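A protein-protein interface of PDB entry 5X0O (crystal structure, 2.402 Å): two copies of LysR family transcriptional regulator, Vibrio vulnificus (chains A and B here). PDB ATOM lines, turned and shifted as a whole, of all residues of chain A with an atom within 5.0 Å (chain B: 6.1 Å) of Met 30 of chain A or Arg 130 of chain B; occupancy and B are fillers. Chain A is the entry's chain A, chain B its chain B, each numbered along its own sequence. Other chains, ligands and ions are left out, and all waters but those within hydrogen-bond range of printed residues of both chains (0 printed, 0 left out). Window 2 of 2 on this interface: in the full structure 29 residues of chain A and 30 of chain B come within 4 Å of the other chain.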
ATOM      1  N   MET A  23     -21.845  16.938 -15.390  1.00  0.00           N
ATOM      2  CA  MET A  23     -21.822  16.539 -13.986  1.00  0.00           C
ATOM      3  C   MET A  23     -20.555  16.953 -13.241  1.00  0.00           C
ATOM      4  O   MET A  23     -20.679  17.382 -12.082  1.00  0.00           O
ATOM      5  CB  MET A  23     -22.056  15.027 -13.874  1.00  0.00           C
ATOM      6  CG  MET A  23     -23.515  14.636 -14.045  1.00  0.00           C
ATOM      7  SD  MET A  23     -24.643  15.684 -13.088  1.00  0.00           S
ATOM      8  CE  MET A  23     -24.101  15.316 -11.419  1.00  0.00           C
ATOM      9  N   LEU A  26     -21.248  20.520 -12.394  1.00  0.00           N
ATOM     10  CA  LEU A  26     -22.353  20.661 -11.450  1.00  0.00           C
ATOM     11  C   LEU A  26     -21.974  20.153 -10.066  1.00  0.00           C
ATOM     12  O   LEU A  26     -22.385  20.728  -9.052  1.00  0.00           O
ATOM     13  CB  LEU A  26     -23.588  19.923 -11.967  1.00  0.00           C
ATOM     14  CG  LEU A  26     -24.193  20.452 -13.267  1.00  0.00           C
ATOM     15  CD1 LEU A  26     -25.391  19.615 -13.685  1.00  0.00           C
ATOM     16  CD2 LEU A  26     -24.587  21.906 -13.106  1.00  0.00           C
ATOM     17  N   ASN A  27     -21.201  19.070 -10.003  1.00  0.00           N
ATOM     18  CA  ASN A  27     -20.747  18.576  -8.709  1.00  0.00           C
ATOM     19  C   ASN A  27     -19.814  19.577  -8.036  1.00  0.00           C
ATOM     20  O   ASN A  27     -19.940  19.841  -6.834  1.00  0.00           O
ATOM     21  CB  ASN A  27     -20.067  17.218  -8.883  1.00  0.00           C
ATOM     22  CG  ASN A  27     -21.064  16.099  -9.122  1.00  0.00           C
ATOM     23  OD1 ASN A  27     -22.194  16.146  -8.629  1.00  0.00           O
ATOM     24  ND2 ASN A  27     -20.651  15.085  -9.875  1.00  0.00           N
ATOM     25  N   GLY A  28     -18.884  20.160  -8.797  1.00  0.00           N
ATOM     26  CA  GLY A  28     -17.982  21.146  -8.227  1.00  0.00           C
ATOM     27  C   GLY A  28     -18.683  22.413  -7.781  1.00  0.00           C
ATOM     28  O   GLY A  28     -18.230  23.079  -6.847  1.00  0.00           O
ATOM     29  N   PHE A  29     -19.787  22.768  -8.441  1.00  0.00           N
ATOM     30  CA  PHE A  29     -20.556  23.932  -8.013  1.00  0.00           C
ATOM     31  C   PHE A  29     -21.318  23.639  -6.728  1.00  0.00           C
ATOM     32  O   PHE A  29     -21.256  24.415  -5.767  1.00  0.00           O
ATOM     33  CB  PHE A  29     -21.523  24.370  -9.112  1.00  0.00           C
ATOM     34  CG  PHE A  29     -22.448  25.475  -8.687  1.00  0.00           C
ATOM     35  CD1 PHE A  29     -22.003  26.787  -8.638  1.00  0.00           C
ATOM     36  CD2 PHE A  29     -23.757  25.203  -8.320  1.00  0.00           C
ATOM     37  CE1 PHE A  29     -22.847  27.806  -8.239  1.00  0.00           C
ATOM     38  CE2 PHE A  29     -24.607  26.223  -7.922  1.00  0.00           C
ATOM     39  CZ  PHE A  29     -24.151  27.524  -7.882  1.00  0.00           C
ATOM     40  N   MET A  30     -22.057  22.526  -6.701  1.00  0.00           N
ATOM     41  CA  MET A  30     -22.785  22.154  -5.494  1.00  0.00           C
ATOM     42  C   MET A  30     -21.844  21.950  -4.320  1.00  0.00           C
ATOM     43  O   MET A  30     -22.199  22.254  -3.176  1.00  0.00           O
ATOM     44  CB  MET A  30     -23.596  20.888  -5.745  1.00  0.00           C
ATOM     45  CG  MET A  30     -24.777  21.098  -6.658  1.00  0.00           C
ATOM     46  SD  MET A  30     -25.812  19.633  -6.720  1.00  0.00           S
ATOM     47  CE  MET A  30     -24.801  18.570  -7.743  1.00  0.00           C
ATOM     48  N   SER A  31     -20.646  21.432  -4.584  1.00  0.00           N
ATOM     49  CA  SER A  31     -19.671  21.249  -3.519  1.00  0.00           C
ATOM     50  C   SER A  31     -19.256  22.587  -2.926  1.00  0.00           C
ATOM     51  O   SER A  31     -19.079  22.708  -1.709  1.00  0.00           O
ATOM     52  CB  SER A  31     -18.461  20.486  -4.056  1.00  0.00           C
ATOM     53  OG  SER A  31     -17.566  20.156  -3.013  1.00  0.00           O
ATOM     54  N   GLN A  32     -19.111  23.609  -3.770  1.00  0.00           N
ATOM     55  CA  GLN A  32     -18.735  24.934  -3.295  1.00  0.00           C
ATOM     56  C   GLN A  32     -19.911  25.703  -2.714  1.00  0.00           C
ATOM     57  O   GLN A  32     -19.701  26.626  -1.920  1.00  0.00           O
ATOM     58  CB  GLN A  32     -18.105  25.742  -4.434  1.00  0.00           C
ATOM     59  CG  GLN A  32     -17.419  27.024  -3.987  1.00  0.00           C
ATOM     60  CD  GLN A  32     -16.913  27.849  -5.152  1.00  0.00           C
ATOM     61  OE1 GLN A  32     -17.200  29.041  -5.253  1.00  0.00           O
ATOM     62  NE2 GLN A  32     -16.147  27.219  -6.036  1.00  0.00           N
ATOM     63  N   TYR A  33     -21.141  25.339  -3.075  1.00  0.00           N
ATOM     64  CA  TYR A  33     -22.341  26.042  -2.626  1.00  0.00           C
ATOM     65  C   TYR A  33     -23.342  25.029  -2.091  1.00  0.00           C
ATOM     66  O   TYR A  33     -24.311  24.670  -2.773  1.00  0.00           O
ATOM     67  CB  TYR A  33     -22.947  26.869  -3.759  1.00  0.00           C
ATOM     68  CG  TYR A  33     -22.037  27.964  -4.260  1.00  0.00           C
ATOM     69  CD1 TYR A  33     -22.076  29.231  -3.700  1.00  0.00           C
ATOM     70  CD2 TYR A  33     -21.135  27.730  -5.290  1.00  0.00           C
ATOM     71  CE1 TYR A  33     -21.248  30.238  -4.153  1.00  0.00           C
ATOM     72  CE2 TYR A  33     -20.302  28.731  -5.751  1.00  0.00           C
ATOM     73  CZ  TYR A  33     -20.363  29.984  -5.177  1.00  0.00           C
ATOM     74  OH  TYR A  33     -19.540  30.989  -5.623  1.00  0.00           O
ATOM     75  N   PRO A  34     -23.141  24.547  -0.863  1.00  0.00           N
ATOM     76  CA  PRO A  34     -24.125  23.623  -0.278  1.00  0.00           C
ATOM     77  C   PRO A  34     -25.469  24.274  -0.007  1.00  0.00           C
ATOM     78  O   PRO A  34     -26.480  23.566   0.062  1.00  0.00           O
ATOM     79  CB  PRO A  34     -23.452  23.164   1.026  1.00  0.00           C
ATOM     80  CG  PRO A  34     -22.012  23.599   0.915  1.00  0.00           C
ATOM     81  CD  PRO A  34     -22.017  24.812   0.049  1.00  0.00           C
ATOM     82  N   ILE A  36     -27.135  26.074  -2.033  1.00  0.00           N
ATOM     83  CA  ILE A  36     -27.887  26.209  -3.274  1.00  0.00           C
ATOM     84  C   ILE A  36     -28.438  24.849  -3.683  1.00  0.00           C
ATOM     85  O   ILE A  36     -27.737  23.832  -3.626  1.00  0.00           O
ATOM     86  CB  ILE A  36     -27.002  26.817  -4.379  1.00  0.00           C
ATOM     87  CG1 ILE A  36     -26.461  28.177  -3.927  1.00  0.00           C
ATOM     88  CG2 ILE A  36     -27.775  26.952  -5.680  1.00  0.00           C
ATOM     89  CD1 ILE A  36     -25.825  28.990  -5.038  1.00  0.00           C
ATOM     90  N   ASN A  37     -29.706  24.828  -4.086  1.00  0.00           N
ATOM     91  CA  ASN A  37     -30.355  23.622  -4.579  1.00  0.00           C
ATOM     92  C   ASN A  37     -30.467  23.687  -6.094  1.00  0.00           C
ATOM     93  O   ASN A  37     -30.727  24.751  -6.665  1.00  0.00           O
ATOM     94  CB  ASN A  37     -31.744  23.445  -3.963  1.00  0.00           C
ATOM     95  CG  ASN A  37     -31.736  23.580  -2.455  1.00  0.00           C
ATOM     96  OD1 ASN A  37     -31.262  22.694  -1.743  1.00  0.00           O
ATOM     97  ND2 ASN A  37     -32.259  24.695  -1.961  1.00  0.00           N
ATOM     98  N   ILE A  38     -30.274  22.543  -6.742  1.00  0.00           N
ATOM     99  CA  ILE A  38     -30.274  22.444  -8.195  1.00  0.00           C
ATOM    100  C   ILE A  38     -31.350  21.454  -8.616  1.00  0.00           C
ATOM    101  O   ILE A  38     -31.458  20.365  -8.039  1.00  0.00           O
ATOM    102  CB  ILE A  38     -28.892  22.020  -8.727  1.00  0.00           C
ATOM    103  CG1 ILE A  38     -27.935  23.212  -8.706  1.00  0.00           C
ATOM    104  CG2 ILE A  38     -29.007  21.431 -10.131  1.00  0.00           C
ATOM    105  CD1 ILE A  38     -26.581  22.919  -9.313  1.00  0.00           C
ATOM    106  N   TYR B  86     -18.952  11.596   2.800  1.00  0.00           N
ATOM    107  CA  TYR B  86     -20.089  12.268   3.420  1.00  0.00           C
ATOM    108  C   TYR B  86     -20.392  11.686   4.793  1.00  0.00           C
ATOM    109  O   TYR B  86     -20.778  12.418   5.712  1.00  0.00           O
ATOM    110  CB  TYR B  86     -21.320  12.172   2.519  1.00  0.00           C
ATOM    111  CG  TYR B  86     -22.540  12.848   3.106  1.00  0.00           C
ATOM    112  CD1 TYR B  86     -22.742  14.210   2.945  1.00  0.00           C
ATOM    113  CD2 TYR B  86     -23.478  12.127   3.836  1.00  0.00           C
ATOM    114  CE1 TYR B  86     -23.848  14.841   3.488  1.00  0.00           C
ATOM    115  CE2 TYR B  86     -24.589  12.749   4.383  1.00  0.00           C
ATOM    116  CZ  TYR B  86     -24.769  14.109   4.203  1.00  0.00           C
ATOM    117  OH  TYR B  86     -25.869  14.743   4.741  1.00  0.00           O
ATOM    118  N   PHE B 103     -28.404  16.507   3.619  1.00  0.00           N
ATOM    119  CA  PHE B 103     -28.538  16.811   2.202  1.00  0.00           C
ATOM    120  C   PHE B 103     -29.091  15.591   1.474  1.00  0.00           C
ATOM    121  O   PHE B 103     -28.575  14.478   1.623  1.00  0.00           O
ATOM    122  CB  PHE B 103     -27.186  17.208   1.605  1.00  0.00           C
ATOM    123  CG  PHE B 103     -26.563  18.423   2.239  1.00  0.00           C
ATOM    124  CD1 PHE B 103     -26.889  19.698   1.797  1.00  0.00           C
ATOM    125  CD2 PHE B 103     -25.635  18.289   3.260  1.00  0.00           C
ATOM    126  CE1 PHE B 103     -26.310  20.818   2.369  1.00  0.00           C
ATOM    127  CE2 PHE B 103     -25.051  19.407   3.837  1.00  0.00           C
ATOM    128  CZ  PHE B 103     -25.389  20.672   3.390  1.00  0.00           C
ATOM    129  N   LEU B 104     -30.140  15.793   0.687  1.00  0.00           N
ATOM    130  CA  LEU B 104     -30.771  14.707  -0.045  1.00  0.00           C
ATOM    131  C   LEU B 104     -30.548  14.887  -1.540  1.00  0.00           C
ATOM    132  O   LEU B 104     -30.551  16.011  -2.051  1.00  0.00           O
ATOM    133  CB  LEU B 104     -32.266  14.633   0.274  1.00  0.00           C
ATOM    134  CG  LEU B 104     -32.585  14.382   1.754  1.00  0.00           C
ATOM    135  CD1 LEU B 104     -34.064  14.097   1.961  1.00  0.00           C
ATOM    136  CD2 LEU B 104     -31.740  13.244   2.315  1.00  0.00           C
ATOM    137  N   LEU B 105     -30.327  13.773  -2.234  1.00  0.00           N
ATOM    138  CA  LEU B 105     -30.177  13.746  -3.683  1.00  0.00           C
ATOM    139  C   LEU B 105     -31.231  12.797  -4.236  1.00  0.00           C
ATOM    140  O   LEU B 105     -31.220  11.605  -3.914  1.00  0.00           O
ATOM    141  CB  LEU B 105     -28.767  13.303  -4.080  1.00  0.00           C
ATOM    142  CG  LEU B 105     -27.628  13.851  -3.208  1.00  0.00           C
ATOM    143  CD1 LEU B 105     -26.356  13.050  -3.405  1.00  0.00           C
ATOM    144  CD2 LEU B 105     -27.364  15.328  -3.477  1.00  0.00           C
ATOM    145  N   ARG B 128     -37.219  18.936  -0.241  1.00  0.00           N
ATOM    146  CA  ARG B 128     -36.461  19.323  -1.419  1.00  0.00           C
ATOM    147  C   ARG B 128     -35.026  18.845  -1.273  1.00  0.00           C
ATOM    148  O   ARG B 128     -34.376  19.092  -0.253  1.00  0.00           O
ATOM    149  CB  ARG B 128     -36.500  20.838  -1.612  1.00  0.00           C
ATOM    150  CG  ARG B 128     -35.784  21.298  -2.870  1.00  0.00           C
ATOM    151  CD  ARG B 128     -35.227  22.700  -2.716  1.00  0.00           C
ATOM    152  NE  ARG B 128     -36.218  23.629  -2.179  1.00  0.00           N
ATOM    153  CZ  ARG B 128     -37.142  24.242  -2.912  1.00  0.00           C
ATOM    154  NH1 ARG B 128     -37.205  24.027  -4.221  1.00  0.00           N
ATOM    155  NH2 ARG B 128     -38.003  25.071  -2.337  1.00  0.00           N
ATOM    156  N   GLY B 129     -34.540  18.134  -2.284  1.00  0.00           N
ATOM    157  CA  GLY B 129     -33.169  17.690  -2.259  1.00  0.00           C
ATOM    158  C   GLY B 129     -32.195  18.810  -2.569  1.00  0.00           C
ATOM    159  O   GLY B 129     -32.547  19.834  -3.154  1.00  0.00           O
ATOM    160  N   ARG B 130     -30.947  18.617  -2.140  1.00  0.00           N
ATOM    161  CA  ARG B 130     -29.883  19.498  -2.603  1.00  0.00           C
ATOM    162  C   ARG B 130     -29.747  19.409  -4.117  1.00  0.00           C
ATOM    163  O   ARG B 130     -29.579  20.426  -4.800  1.00  0.00           O
ATOM    164  CB  ARG B 130     -28.564  19.142  -1.910  1.00  0.00           C
ATOM    165  CG  ARG B 130     -27.357  19.923  -2.407  1.00  0.00           C
ATOM    166  CD  ARG B 130     -26.079  19.108  -2.286  1.00  0.00           C
ATOM    167  NE  ARG B 130     -24.904  19.955  -2.088  1.00  0.00           N
ATOM    168  CZ  ARG B 130     -24.003  19.764  -1.130  1.00  0.00           C
ATOM    169  NH1 ARG B 130     -24.144  18.757  -0.279  1.00  0.00           N
ATOM    170  NH2 ARG B 130     -22.963  20.580  -1.018  1.00  0.00           N
ATOM    171  N   PHE B 131     -29.864  18.199  -4.661  1.00  0.00           N
ATOM    172  CA  PHE B 131     -29.823  17.943  -6.093  1.00  0.00           C
ATOM    173  C   PHE B 131     -31.027  17.088  -6.460  1.00  0.00           C
ATOM    174  O   PHE B 131     -31.251  16.035  -5.853  1.00  0.00           O
ATOM    175  CB  PHE B 131     -28.510  17.237  -6.487  1.00  0.00           C
ATOM    176  CG  PHE B 131     -28.349  17.018  -7.969  1.00  0.00           C
ATOM    177  CD1 PHE B 131     -27.978  15.776  -8.462  1.00  0.00           C
ATOM    178  CD2 PHE B 131     -28.573  18.048  -8.865  1.00  0.00           C
ATOM    179  CE1 PHE B 131     -27.825  15.572  -9.832  1.00  0.00           C
ATOM    180  CE2 PHE B 131     -28.425  17.851 -10.230  1.00  0.00           C
ATOM    181  CZ  PHE B 131     -28.050  16.610 -10.714  1.00  0.00           C
ATOM    182  N   GLN B 132     -31.801  17.540  -7.441  1.00  0.00           N
ATOM    183  CA  GLN B 132     -32.928  16.780  -7.963  1.00  0.00           C
ATOM    184  C   GLN B 132     -32.802  16.681  -9.474  1.00  0.00           C
ATOM    185  O   GLN B 132     -32.438  17.655 -10.139  1.00  0.00           O
ATOM    186  CB  GLN B 132     -34.266  17.421  -7.583  1.00  0.00           C
ATOM    187  CG  GLN B 132     -34.570  17.373  -6.095  1.00  0.00           C
ATOM    188  CD  GLN B 132     -36.028  17.650  -5.781  1.00  0.00           C
ATOM    189  OE1 GLN B 132     -36.439  17.606  -4.622  1.00  0.00           O
ATOM    190  NE2 GLN B 132     -36.815  17.943  -6.812  1.00  0.00           N
ATOM    191  N   ALA B 142     -23.525  12.389  -8.156  1.00  0.00           N
ATOM    192  CA  ALA B 142     -23.415  13.381  -7.093  1.00  0.00           C
ATOM    193  C   ALA B 142     -23.276  12.721  -5.730  1.00  0.00           C
ATOM    194  O   ALA B 142     -22.619  13.273  -4.840  1.00  0.00           O
ATOM    195  CB  ALA B 142     -24.625  14.313  -7.109  1.00  0.00           C
ATOM    196  N   GLY B 146     -19.989  12.676  -2.571  1.00  0.00           N
ATOM    197  CA  GLY B 146     -20.190  13.027  -1.179  1.00  0.00           C
ATOM    198  C   GLY B 146     -21.118  14.193  -0.934  1.00  0.00           C
ATOM    199  O   GLY B 146     -20.994  14.867   0.093  1.00  0.00           O
ATOM    200  N   LEU B 147     -22.062  14.445  -1.839  1.00  0.00           N
ATOM    201  CA  LEU B 147     -22.951  15.591  -1.717  1.00  0.00           C
ATOM    202  C   LEU B 147     -24.240  15.286  -0.962  1.00  0.00           C
ATOM    203  O   LEU B 147     -25.111  16.158  -0.887  1.00  0.00           O
ATOM    204  CB  LEU B 147     -23.289  16.153  -3.101  1.00  0.00           C
ATOM    205  CG  LEU B 147     -22.068  16.590  -3.911  1.00  0.00           C
ATOM    206  CD1 LEU B 147     -22.468  17.001  -5.321  1.00  0.00           C
ATOM    207  CD2 LEU B 147     -21.333  17.711  -3.199  1.00  0.00           C
ATOM    208  N   GLY B 148     -24.385  14.097  -0.392  1.00  0.00           N
ATOM    209  CA  GLY B 148     -25.530  13.801   0.444  1.00  0.00           C
ATOM    210  C   GLY B 148     -25.983  12.361   0.292  1.00  0.00           C
ATOM    211  O   GLY B 148     -25.273  11.516  -0.247  1.00  0.00           O
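The backbone carbonyl oxygen (O) of Met 23 of chain A is in hydrogen-bond range of the side-chain amide nitrogen (ND2) of Asn 27 of chain A, 3.2 Å away.
OH of Tyr 86 of chain B lies within hydrogen-bond range of N of Phe 103 of chain B (3.3 Å).
The backbone carbonyl oxygen (O) of Leu 104 of chain B sits at hydrogen-bond distance from the backbone NH (N) of Arg 130 of chain B (2.6 Å).
The backbone NH of Phe 131 of chain B lies within hydrogen-bond range of the backbone carbonyl oxygen of Leu 104 of chain B.
N of Gly 129 of chain B sits at hydrogen-bond distance from OE1 of Gln 132 of chain B.
O of Leu 147 of chain B sits at hydrogen-bond distance from NH1 of Arg 130 of chain B, 2.8 Å away.
Among the printed residues, merely in contact across the chains: Asn 27 of chain A with Ala 142 of chain B (3.4 Å), Asn 27 of chain A with Leu 147 of chain B (3.4 Å), Met 30 of chain A with Phe 131 of chain B (3.6 Å), Met 30 of chain A with Leu 147 of chain B (3.7 Å), Ser 31 of chain A with Leu 147 of chain B (3.9 Å), Pro 34 of chain A with Phe 103 of chain B (3.6 Å), Pro 34 of chain A with Arg 130 of chain B (3.3 Å), Asn 37 of chain A with Arg 128 of chain B (3.6 Å), Asn 37 of chain A with Arg 130 of chain B (3.3 Å) and Ile 38 of chain A with Phe 131 of chain B (3.5 Å).
No position is printed for both chains.
Of the 13 printed residues of chain B, 8 touch a printed residue of chain A.
Printed residues of chain B that touch a printed residue of chain A: Phe 103, Arg 128, Gly 129, Arg 130, Phe 131, Gln 132, Ala 142 and Leu 147.
Hydrophobic or aromatic side chains of chain B that line the printed part of chain A: Phe 103, Phe 131, Ala 142 and Leu 147.
Of the 13 printed residues of chain A, 6 touch a printed residue of chain B.
Hydrophobic or aromatic side chains of chain A within 4 Å of the printed part of chain B: Met 30, Pro 34 and Ile 38.
Among the printed residues, 14 pairs touch across the chains.
Arg 130 of chain B touches four residues of chain A.
Of the printed residues of chain A, Arg 128 of chain B touches Asn 37 (3.6 Å).
Printed residues of chain A within 4 Å of Gln 132 of chain B: Ile 38.
Of the printed residues of chain A, Leu 147 of chain B touches Asn 27, Met 30 and Ser 31.
Of the printed residues of chain A, Phe 131 of chain B touches Met 30 (3.6 Å) and Ile 38 (3.5 Å).
The nearest residue of chain A that does not touch Arg 130 of chain B is Ile 36 of chain A (4.05 Å).
The nearest printed residue of chain A that does not touch Gln 132 of chain B is Met 30 of chain A (6.4 Å).
The backbone carbonyl oxygen of Met 30 of chain A is in hydrogen-bond range of the guanidinium group of Arg 130 of chain B, at 2.8 Å.
OD1 of Asn 37 of chain A lies close to O of Gly 129 of chain B.
N of Ile 38 of chain A lies within hydrogen-bond range of O of Arg 130 of chain B (3.0 Å).
N of Gln 132 of chain B sits at hydrogen-bond distance from O of Ile 38 of chain A, at 2.9 Å.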
